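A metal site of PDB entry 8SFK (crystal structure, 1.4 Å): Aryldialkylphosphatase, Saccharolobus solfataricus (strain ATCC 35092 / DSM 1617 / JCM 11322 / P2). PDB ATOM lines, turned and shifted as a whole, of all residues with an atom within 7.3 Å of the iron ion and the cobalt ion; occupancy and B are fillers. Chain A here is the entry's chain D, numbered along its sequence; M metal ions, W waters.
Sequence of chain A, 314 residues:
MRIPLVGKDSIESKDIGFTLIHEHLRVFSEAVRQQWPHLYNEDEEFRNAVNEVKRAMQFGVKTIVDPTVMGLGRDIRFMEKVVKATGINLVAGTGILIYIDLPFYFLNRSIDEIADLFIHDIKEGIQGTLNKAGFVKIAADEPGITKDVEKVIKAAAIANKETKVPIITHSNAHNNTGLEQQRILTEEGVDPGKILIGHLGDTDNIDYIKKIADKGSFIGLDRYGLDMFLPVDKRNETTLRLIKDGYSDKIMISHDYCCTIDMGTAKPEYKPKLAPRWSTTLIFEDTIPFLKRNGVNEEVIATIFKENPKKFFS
O of Pro 67 lies within hydrogen-bond range of NZ of KCX 137 (3.5 Å). The backbone NH of His 24 is in hydrogen-bond range of the backbone carbonyl oxygen of Tyr 257 (2.8 Å). A ring nitrogen (NE2) of His 170 lies within hydrogen-bond range of the side-chain hydroxyl of Tyr 99 (3.1 Å). OD2 of Asp 141 lies within hydrogen-bond range of NE2 of His 170 (2.8 Å). The backbone NH of His 170 is in hydrogen-bond range of the backbone carbonyl oxygen of Ile 138 (2.9 Å). OD2 of Asp 256 is in salt-bridge range of NE of Arg 223 (2.9 Å). O of Asp 256 lies within hydrogen-bond range of SG of Cys 258 (3.7 Å). N of Asp 256 lies within hydrogen-bond range of O of Asp 222.
Within 4 Å of the iron ion: His 22, His 24, KCX 137 and Asp 256.
NH2 of Arg 223 touches the cobalt ion (3.7 Å). The nearest printed residue that does not touch the cobalt ion is Asp 256 (4.1 Å).
The iron ion is bound by water W1 (1.9 Å), a ring nitrogen (NE2) of His 24 (2.1 Å), OQ1 of KCX 137 (2.1 Å), a ring nitrogen (NE2) of His 22 (2.1 Å) and the side-chain carboxylate (OD1) of Asp 256 (2.2 Å).
Water W1 binds the cobalt ion, 1.9 Å away. The cobalt ion is bound by OQ2 of KCX 137 (2.1 Å). ND1 of His 170 binds the cobalt ion (2.1 Å). A ring nitrogen (NE2) of His 199 binds the cobalt ion, at 2.1 Å.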
ATOM      1  N   HIS A  22     -23.874 -19.375 -12.990  1.00  0.00           N
ATOM      2  CA  HIS A  22     -25.101 -18.995 -12.268  1.00  0.00           C
ATOM      3  C   HIS A  22     -25.881 -17.985 -13.102  1.00  0.00           C
ATOM      4  O   HIS A  22     -25.696 -16.768 -12.947  1.00  0.00           O
ATOM      5  CB  HIS A  22     -24.768 -18.470 -10.877  1.00  0.00           C
ATOM      6  CG  HIS A  22     -25.960 -18.330  -9.975  1.00  0.00           C
ATOM      7  ND1 HIS A  22     -25.941 -18.724  -8.653  1.00  0.00           N
ATOM      8  CD2 HIS A  22     -27.204 -17.838 -10.197  1.00  0.00           C
ATOM      9  CE1 HIS A  22     -27.111 -18.486  -8.104  1.00  0.00           C
ATOM     10  NE2 HIS A  22     -27.896 -17.945  -9.009  1.00  0.00           N
ATOM     11  N   GLU A  23     -26.761 -18.485 -13.970  1.00  0.00           N
ATOM     12  CA  GLU A  23     -27.675 -17.659 -14.763  1.00  0.00           C
ATOM     13  C   GLU A  23     -29.031 -18.344 -14.818  1.00  0.00           C
ATOM     14  O   GLU A  23     -29.111 -19.560 -14.667  1.00  0.00           O
ATOM     15  CB  GLU A  23     -27.154 -17.474 -16.212  1.00  0.00           C
ATOM     16  CG  GLU A  23     -25.661 -17.082 -16.291  1.00  0.00           C
ATOM     17  CD  GLU A  23     -25.376 -15.656 -15.838  1.00  0.00           C
ATOM     18  OE1 GLU A  23     -24.196 -15.347 -15.571  1.00  0.00           O
ATOM     19  OE2 GLU A  23     -26.325 -14.851 -15.754  1.00  0.00           O
ATOM     20  N   HIS A  24     -30.091 -17.561 -15.017  1.00  0.00           N
ATOM     21  CA  HIS A  24     -31.454 -18.097 -15.019  1.00  0.00           C
ATOM     22  C   HIS A  24     -32.126 -17.818 -16.348  1.00  0.00           C
ATOM     23  O   HIS A  24     -32.303 -16.650 -16.725  1.00  0.00           O
ATOM     24  CB  HIS A  24     -32.310 -17.450 -13.916  1.00  0.00           C
ATOM     25  CG  HIS A  24     -31.808 -17.710 -12.520  1.00  0.00           C
ATOM     26  ND1 HIS A  24     -32.170 -18.823 -11.804  1.00  0.00           N
ATOM     27  CD2 HIS A  24     -30.994 -16.983 -11.714  1.00  0.00           C
ATOM     28  CE1 HIS A  24     -31.602 -18.773 -10.615  1.00  0.00           C
ATOM     29  NE2 HIS A  24     -30.886 -17.663 -10.514  1.00  0.00           N
ATOM     30  N   VAL A  27     -37.313 -17.043 -14.232  1.00  0.00           N
ATOM     31  CA  VAL A  27     -37.709 -17.225 -12.836  1.00  0.00           C
ATOM     32  C   VAL A  27     -39.158 -16.795 -12.652  1.00  0.00           C
ATOM     33  O   VAL A  27     -39.591 -15.764 -13.185  1.00  0.00           O
ATOM     34  CB  VAL A  27     -36.794 -16.404 -11.898  1.00  0.00           C
ATOM     35  CG1 VAL A  27     -37.350 -16.387 -10.489  1.00  0.00           C
ATOM     36  CG2 VAL A  27     -35.385 -16.979 -11.929  1.00  0.00           C
ATOM     37  N   ASP A  66     -27.767 -23.381 -14.741  1.00  0.00           N
ATOM     38  CA  ASP A  66     -28.975 -22.647 -14.399  1.00  0.00           C
ATOM     39  C   ASP A  66     -29.541 -23.199 -13.098  1.00  0.00           C
ATOM     40  O   ASP A  66     -30.136 -24.286 -13.099  1.00  0.00           O
ATOM     41  CB  ASP A  66     -29.997 -22.776 -15.525  1.00  0.00           C
ATOM     42  CG  ASP A  66     -31.286 -22.004 -15.275  1.00  0.00           C
ATOM     43  OD1 ASP A  66     -31.612 -21.749 -14.095  1.00  0.00           O
ATOM     44  OD2 ASP A  66     -32.000 -21.645 -16.240  1.00  0.00           O
ATOM     45  N   PRO A  67     -29.393 -22.490 -11.963  1.00  0.00           N
ATOM     46  CA  PRO A  67     -29.830 -23.047 -10.678  1.00  0.00           C
ATOM     47  C   PRO A  67     -31.262 -22.663 -10.322  1.00  0.00           C
ATOM     48  O   PRO A  67     -31.577 -22.487  -9.134  1.00  0.00           O
ATOM     49  CB  PRO A  67     -28.804 -22.463  -9.699  1.00  0.00           C
ATOM     50  CG  PRO A  67     -28.472 -21.131 -10.271  1.00  0.00           C
ATOM     51  CD  PRO A  67     -28.584 -21.270 -11.802  1.00  0.00           C
ATOM     52  N   THR A  68     -32.135 -22.551 -11.325  1.00  0.00           N
ATOM     53  CA  THR A  68     -33.566 -22.403 -11.086  1.00  0.00           C
ATOM     54  C   THR A  68     -34.110 -23.724 -10.576  1.00  0.00           C
ATOM     55  O   THR A  68     -34.034 -24.746 -11.266  1.00  0.00           O
ATOM     56  CB  THR A  68     -34.282 -22.019 -12.387  1.00  0.00           C
ATOM     57  OG1 THR A  68     -33.650 -20.876 -12.974  1.00  0.00           O
ATOM     58  CG2 THR A  68     -35.740 -21.686 -12.115  1.00  0.00           C
ATOM     59  N   LEU A  72     -38.284 -21.055  -7.574  1.00  0.00           N
ATOM     60  CA  LEU A  72     -37.911 -20.148  -8.658  1.00  0.00           C
ATOM     61  C   LEU A  72     -38.546 -20.529  -9.992  1.00  0.00           C
ATOM     62  O   LEU A  72     -38.268 -19.881 -11.005  1.00  0.00           O
ATOM     63  CB  LEU A  72     -36.391 -20.065  -8.797  1.00  0.00           C
ATOM     64  CG  LEU A  72     -35.608 -19.626  -7.556  1.00  0.00           C
ATOM     65  CD1 LEU A  72     -34.137 -19.746  -7.854  1.00  0.00           C
ATOM     66  CD2 LEU A  72     -35.993 -18.214  -7.181  1.00  0.00           C
ATOM     67  N   LEU A  97     -35.279 -23.610  -2.977  1.00  0.00           N
ATOM     68  CA  LEU A  97     -34.903 -22.263  -2.542  1.00  0.00           C
ATOM     69  C   LEU A  97     -36.007 -21.760  -1.616  1.00  0.00           C
ATOM     70  O   LEU A  97     -37.093 -21.404  -2.068  1.00  0.00           O
ATOM     71  CB  LEU A  97     -34.724 -21.327  -3.746  1.00  0.00           C
ATOM     72  CG  LEU A  97     -34.096 -20.008  -3.265  1.00  0.00           C
ATOM     73  CD1 LEU A  97     -32.903 -19.593  -4.107  1.00  0.00           C
ATOM     74  CD2 LEU A  97     -35.125 -18.897  -3.171  1.00  0.00           C
ATOM     75  N   TYR A  99     -36.356 -19.270   2.225  1.00  0.00           N
ATOM     76  CA  TYR A  99     -35.708 -18.448   3.234  1.00  0.00           C
ATOM     77  C   TYR A  99     -36.210 -18.721   4.646  1.00  0.00           C
ATOM     78  O   TYR A  99     -35.474 -18.443   5.597  1.00  0.00           O
ATOM     79  CB  TYR A  99     -35.914 -16.957   2.957  1.00  0.00           C
ATOM     80  CG  TYR A  99     -35.286 -16.394   1.688  1.00  0.00           C
ATOM     81  CD1 TYR A  99     -34.474 -17.168   0.866  1.00  0.00           C
ATOM     82  CD2 TYR A  99     -35.506 -15.076   1.341  1.00  0.00           C
ATOM     83  CE1 TYR A  99     -33.911 -16.629  -0.304  1.00  0.00           C
ATOM     84  CE2 TYR A  99     -34.959 -14.522   0.192  1.00  0.00           C
ATOM     85  CZ  TYR A  99     -34.163 -15.301  -0.634  1.00  0.00           C
ATOM     86  OH  TYR A  99     -33.618 -14.733  -1.765  1.00  0.00           O
ATOM     87  N   KCX A 137     -29.133 -27.200  -5.523  1.00  0.00           N
ATOM     88  CA  KCX A 137     -29.191 -25.792  -5.146  1.00  0.00           C
ATOM     89  CB  KCX A 137     -29.906 -24.998  -6.248  1.00  0.00           C
ATOM     90  CG  KCX A 137     -30.225 -23.543  -5.922  1.00  0.00           C
ATOM     91  CD  KCX A 137     -28.974 -22.699  -5.754  1.00  0.00           C
ATOM     92  CE  KCX A 137     -29.323 -21.249  -5.451  1.00  0.00           C
ATOM     93  NZ  KCX A 137     -29.984 -20.627  -6.644  1.00  0.00           N
ATOM     94  C   KCX A 137     -29.949 -25.633  -3.835  1.00  0.00           C
ATOM     95  O   KCX A 137     -31.046 -26.188  -3.676  1.00  0.00           O
ATOM     96  CX  KCX A 137     -30.012 -19.305  -6.783  1.00  0.00           C
ATOM     97  OQ1 KCX A 137     -30.582 -18.811  -7.782  1.00  0.00           O
ATOM     98  OQ2 KCX A 137     -29.478 -18.576  -5.901  1.00  0.00           O
ATOM     99  N   ILE A 138     -29.351 -24.887  -2.891  1.00  0.00           N
ATOM    100  CA  ILE A 138     -29.973 -24.585  -1.592  1.00  0.00           C
ATOM    101  C   ILE A 138     -29.813 -23.113  -1.277  1.00  0.00           C
ATOM    102  O   ILE A 138     -29.022 -22.417  -1.929  1.00  0.00           O
ATOM    103  CB  ILE A 138     -29.415 -25.468  -0.449  1.00  0.00           C
ATOM    104  CG1 ILE A 138     -27.940 -25.153  -0.163  1.00  0.00           C
ATOM    105  CG2 ILE A 138     -29.593 -26.947  -0.777  1.00  0.00           C
ATOM    106  CD1 ILE A 138     -27.709 -24.179   0.982  1.00  0.00           C
ATOM    107  N   ALA A 139     -30.544 -22.617  -0.273  1.00  0.00           N
ATOM    108  CA  ALA A 139     -30.530 -21.191   0.028  1.00  0.00           C
ATOM    109  C   ALA A 139     -30.594 -20.907   1.520  1.00  0.00           C
ATOM    110  O   ALA A 139     -31.026 -21.728   2.327  1.00  0.00           O
ATOM    111  CB  ALA A 139     -31.711 -20.451  -0.623  1.00  0.00           C
ATOM    112  N   ASP A 141     -31.039 -16.741   3.651  1.00  0.00           N
ATOM    113  CA  ASP A 141     -30.942 -15.310   3.438  1.00  0.00           C
ATOM    114  C   ASP A 141     -31.044 -14.588   4.770  1.00  0.00           C
ATOM    115  O   ASP A 141     -30.537 -15.092   5.782  1.00  0.00           O
ATOM    116  CB  ASP A 141     -31.979 -14.838   2.415  1.00  0.00           C
ATOM    117  CG  ASP A 141     -31.560 -13.567   1.672  1.00  0.00           C
ATOM    118  OD1 ASP A 141     -31.640 -12.478   2.279  1.00  0.00           O
ATOM    119  OD2 ASP A 141     -31.136 -13.647   0.500  1.00  0.00           O
ATOM    120  N   THR A 169     -24.999 -22.727  -3.683  1.00  0.00           N
ATOM    121  CA  THR A 169     -25.853 -22.054  -2.714  1.00  0.00           C
ATOM    122  C   THR A 169     -26.197 -20.624  -3.127  1.00  0.00           C
ATOM    123  O   THR A 169     -25.500 -19.968  -3.914  1.00  0.00           O
ATOM    124  CB  THR A 169     -25.272 -22.021  -1.274  1.00  0.00           C
ATOM    125  OG1 THR A 169     -24.431 -20.870  -1.106  1.00  0.00           O
ATOM    126  CG2 THR A 169     -24.501 -23.283  -0.941  1.00  0.00           C
ATOM    127  N   HIS A 170     -27.323 -20.181  -2.575  1.00  0.00           N
ATOM    128  CA  HIS A 170     -27.702 -18.791  -2.440  1.00  0.00           C
ATOM    129  C   HIS A 170     -27.461 -18.417  -0.991  1.00  0.00           C
ATOM    130  O   HIS A 170     -27.921 -19.128  -0.086  1.00  0.00           O
ATOM    131  CB  HIS A 170     -29.199 -18.674  -2.742  1.00  0.00           C
ATOM    132  CG  HIS A 170     -29.805 -17.338  -2.434  1.00  0.00           C
ATOM    133  ND1 HIS A 170     -30.258 -16.478  -3.409  1.00  0.00           N
ATOM    134  CD2 HIS A 170     -30.049 -16.727  -1.248  1.00  0.00           C
ATOM    135  CE1 HIS A 170     -30.764 -15.394  -2.835  1.00  0.00           C
ATOM    136  NE2 HIS A 170     -30.646 -15.520  -1.522  1.00  0.00           N
ATOM    137  N   SER A 171     -26.737 -17.335  -0.746  1.00  0.00           N
ATOM    138  CA  SER A 171     -26.568 -16.834   0.617  1.00  0.00           C
ATOM    139  C   SER A 171     -26.781 -15.319   0.624  1.00  0.00           C
ATOM    140  O   SER A 171     -26.907 -14.683  -0.426  1.00  0.00           O
ATOM    141  CB  SER A 171     -25.204 -17.226   1.222  1.00  0.00           C
ATOM    142  OG  SER A 171     -24.154 -16.339   0.848  1.00  0.00           O
ATOM    143  N   GLY A 198     -22.739 -18.970  -2.692  1.00  0.00           N
ATOM    144  CA  GLY A 198     -23.214 -17.964  -3.619  1.00  0.00           C
ATOM    145  C   GLY A 198     -23.393 -16.578  -3.038  1.00  0.00           C
ATOM    146  O   GLY A 198     -23.578 -16.373  -1.835  1.00  0.00           O
ATOM    147  N   HIS A 199     -23.313 -15.603  -3.945  1.00  0.00           N
ATOM    148  CA  HIS A 199     -23.653 -14.209  -3.712  1.00  0.00           C
ATOM    149  C   HIS A 199     -22.652 -13.475  -2.832  1.00  0.00           C
ATOM    150  O   HIS A 199     -22.947 -12.409  -2.294  1.00  0.00           O
ATOM    151  CB  HIS A 199     -25.107 -14.028  -3.241  1.00  0.00           C
ATOM    152  CG  HIS A 199     -26.105 -14.711  -4.131  1.00  0.00           C
ATOM    153  ND1 HIS A 199     -25.892 -14.908  -5.481  1.00  0.00           N
ATOM    154  CD2 HIS A 199     -27.324 -15.235  -3.868  1.00  0.00           C
ATOM    155  CE1 HIS A 199     -26.926 -15.552  -5.994  1.00  0.00           C
ATOM    156  NE2 HIS A 199     -27.811 -15.758  -5.043  1.00  0.00           N
ATOM    157  N   ASP A 222     -21.025 -13.486  -8.225  1.00  0.00           N
ATOM    158  CA  ASP A 222     -21.967 -14.077  -9.172  1.00  0.00           C
ATOM    159  C   ASP A 222     -23.165 -13.202  -9.501  1.00  0.00           C
ATOM    160  O   ASP A 222     -24.133 -13.697 -10.085  1.00  0.00           O
ATOM    161  CB  ASP A 222     -22.398 -15.467  -8.680  1.00  0.00           C
ATOM    162  CG  ASP A 222     -23.047 -15.437  -7.304  1.00  0.00           C
ATOM    163  OD1 ASP A 222     -23.499 -14.361  -6.890  1.00  0.00           O
ATOM    164  OD2 ASP A 222     -23.112 -16.501  -6.657  1.00  0.00           O
ATOM    165  N   ARG A 223     -23.134 -11.908  -9.173  1.00  0.00           N
ATOM    166  CA  ARG A 223     -24.264 -11.024  -9.403  1.00  0.00           C
ATOM    167  C   ARG A 223     -23.837  -9.760 -10.123  1.00  0.00           C
ATOM    168  O   ARG A 223     -24.387  -8.670  -9.899  1.00  0.00           O
ATOM    169  CB  ARG A 223     -25.021 -10.712  -8.111  1.00  0.00           C
ATOM    170  CG  ARG A 223     -25.934 -11.853  -7.708  1.00  0.00           C
ATOM    171  CD  ARG A 223     -26.603 -11.557  -6.369  1.00  0.00           C
ATOM    172  NE  ARG A 223     -27.901 -12.212  -6.285  1.00  0.00           N
ATOM    173  CZ  ARG A 223     -28.633 -12.263  -5.177  1.00  0.00           C
ATOM    174  NH1 ARG A 223     -28.195 -11.694  -4.063  1.00  0.00           N
ATOM    175  NH2 ARG A 223     -29.806 -12.887  -5.191  1.00  0.00           N
ATOM    176  N   HIS A 255     -23.501 -13.599 -13.462  1.00  0.00           N
ATOM    177  CA  HIS A 255     -24.362 -12.432 -13.376  1.00  0.00           C
ATOM    178  C   HIS A 255     -25.645 -12.664 -12.605  1.00  0.00           C
ATOM    179  O   HIS A 255     -26.285 -11.670 -12.223  1.00  0.00           O
ATOM    180  CB  HIS A 255     -24.766 -11.907 -14.767  1.00  0.00           C
ATOM    181  CG  HIS A 255     -23.626 -11.774 -15.734  1.00  0.00           C
ATOM    182  ND1 HIS A 255     -23.202 -12.827 -16.520  1.00  0.00           N
ATOM    183  CD2 HIS A 255     -22.875 -10.710 -16.087  1.00  0.00           C
ATOM    184  CE1 HIS A 255     -22.222 -12.410 -17.307  1.00  0.00           C
ATOM    185  NE2 HIS A 255     -22.003 -11.133 -17.065  1.00  0.00           N
ATOM    186  N   ASP A 256     -26.078 -13.906 -12.423  1.00  0.00           N
ATOM    187  CA  ASP A 256     -27.391 -14.182 -11.839  1.00  0.00           C
ATOM    188  C   ASP A 256     -28.484 -13.551 -12.686  1.00  0.00           C
ATOM    189  O   ASP A 256     -29.555 -13.186 -12.176  1.00  0.00           O
ATOM    190  CB  ASP A 256     -27.468 -13.686 -10.386  1.00  0.00           C
ATOM    191  CG  ASP A 256     -28.532 -14.397  -9.563  1.00  0.00           C
ATOM    192  OD1 ASP A 256     -29.088 -15.417 -10.022  1.00  0.00           O
ATOM    193  OD2 ASP A 256     -28.785 -13.922  -8.430  1.00  0.00           O
ATOM    194  N   TYR A 257     -28.234 -13.395 -13.981  1.00  0.00           N
ATOM    195  CA  TYR A 257     -29.178 -12.698 -14.824  1.00  0.00           C
ATOM    196  C   TYR A 257     -30.418 -13.545 -14.983  1.00  0.00           C
ATOM    197  O   TYR A 257     -30.345 -14.770 -15.124  1.00  0.00           O
ATOM    198  CB  TYR A 257     -28.590 -12.386 -16.200  1.00  0.00           C
ATOM    199  CG  TYR A 257     -29.537 -11.539 -17.025  1.00  0.00           C
ATOM    200  CD1 TYR A 257     -29.878 -10.258 -16.608  1.00  0.00           C
ATOM    201  CD2 TYR A 257     -30.102 -12.028 -18.189  1.00  0.00           C
ATOM    202  CE1 TYR A 257     -30.749  -9.485 -17.336  1.00  0.00           C
ATOM    203  CE2 TYR A 257     -30.976 -11.259 -18.926  1.00  0.00           C
ATOM    204  CZ  TYR A 257     -31.300  -9.988 -18.499  1.00  0.00           C
ATOM    205  OH  TYR A 257     -32.169  -9.229 -19.244  1.00  0.00           O
ATOM    206  N   CYS A 258     -31.567 -12.899 -14.949  1.00  0.00           N
ATOM    207  CA  CYS A 258     -32.836 -13.569 -15.174  1.00  0.00           C
ATOM    208  C   CYS A 258     -33.384 -13.036 -16.478  1.00  0.00           C
ATOM    209  O   CYS A 258     -33.752 -11.861 -16.572  1.00  0.00           O
ATOM    210  CB  CYS A 258     -33.801 -13.305 -14.022  1.00  0.00           C
ATOM    211  SG  CYS A 258     -33.185 -13.896 -12.433  1.00  0.00           S
HETATM  212 FE    FE M   1     -29.855 -17.109  -8.790  1.00  0.00          FE
HETATM  213 CO    CO M   2     -29.720 -16.581  -5.442  1.00  0.00          CO
HETATM  214  O   HOH W   1     -29.944 -15.961  -7.223  1.00  0.00           O
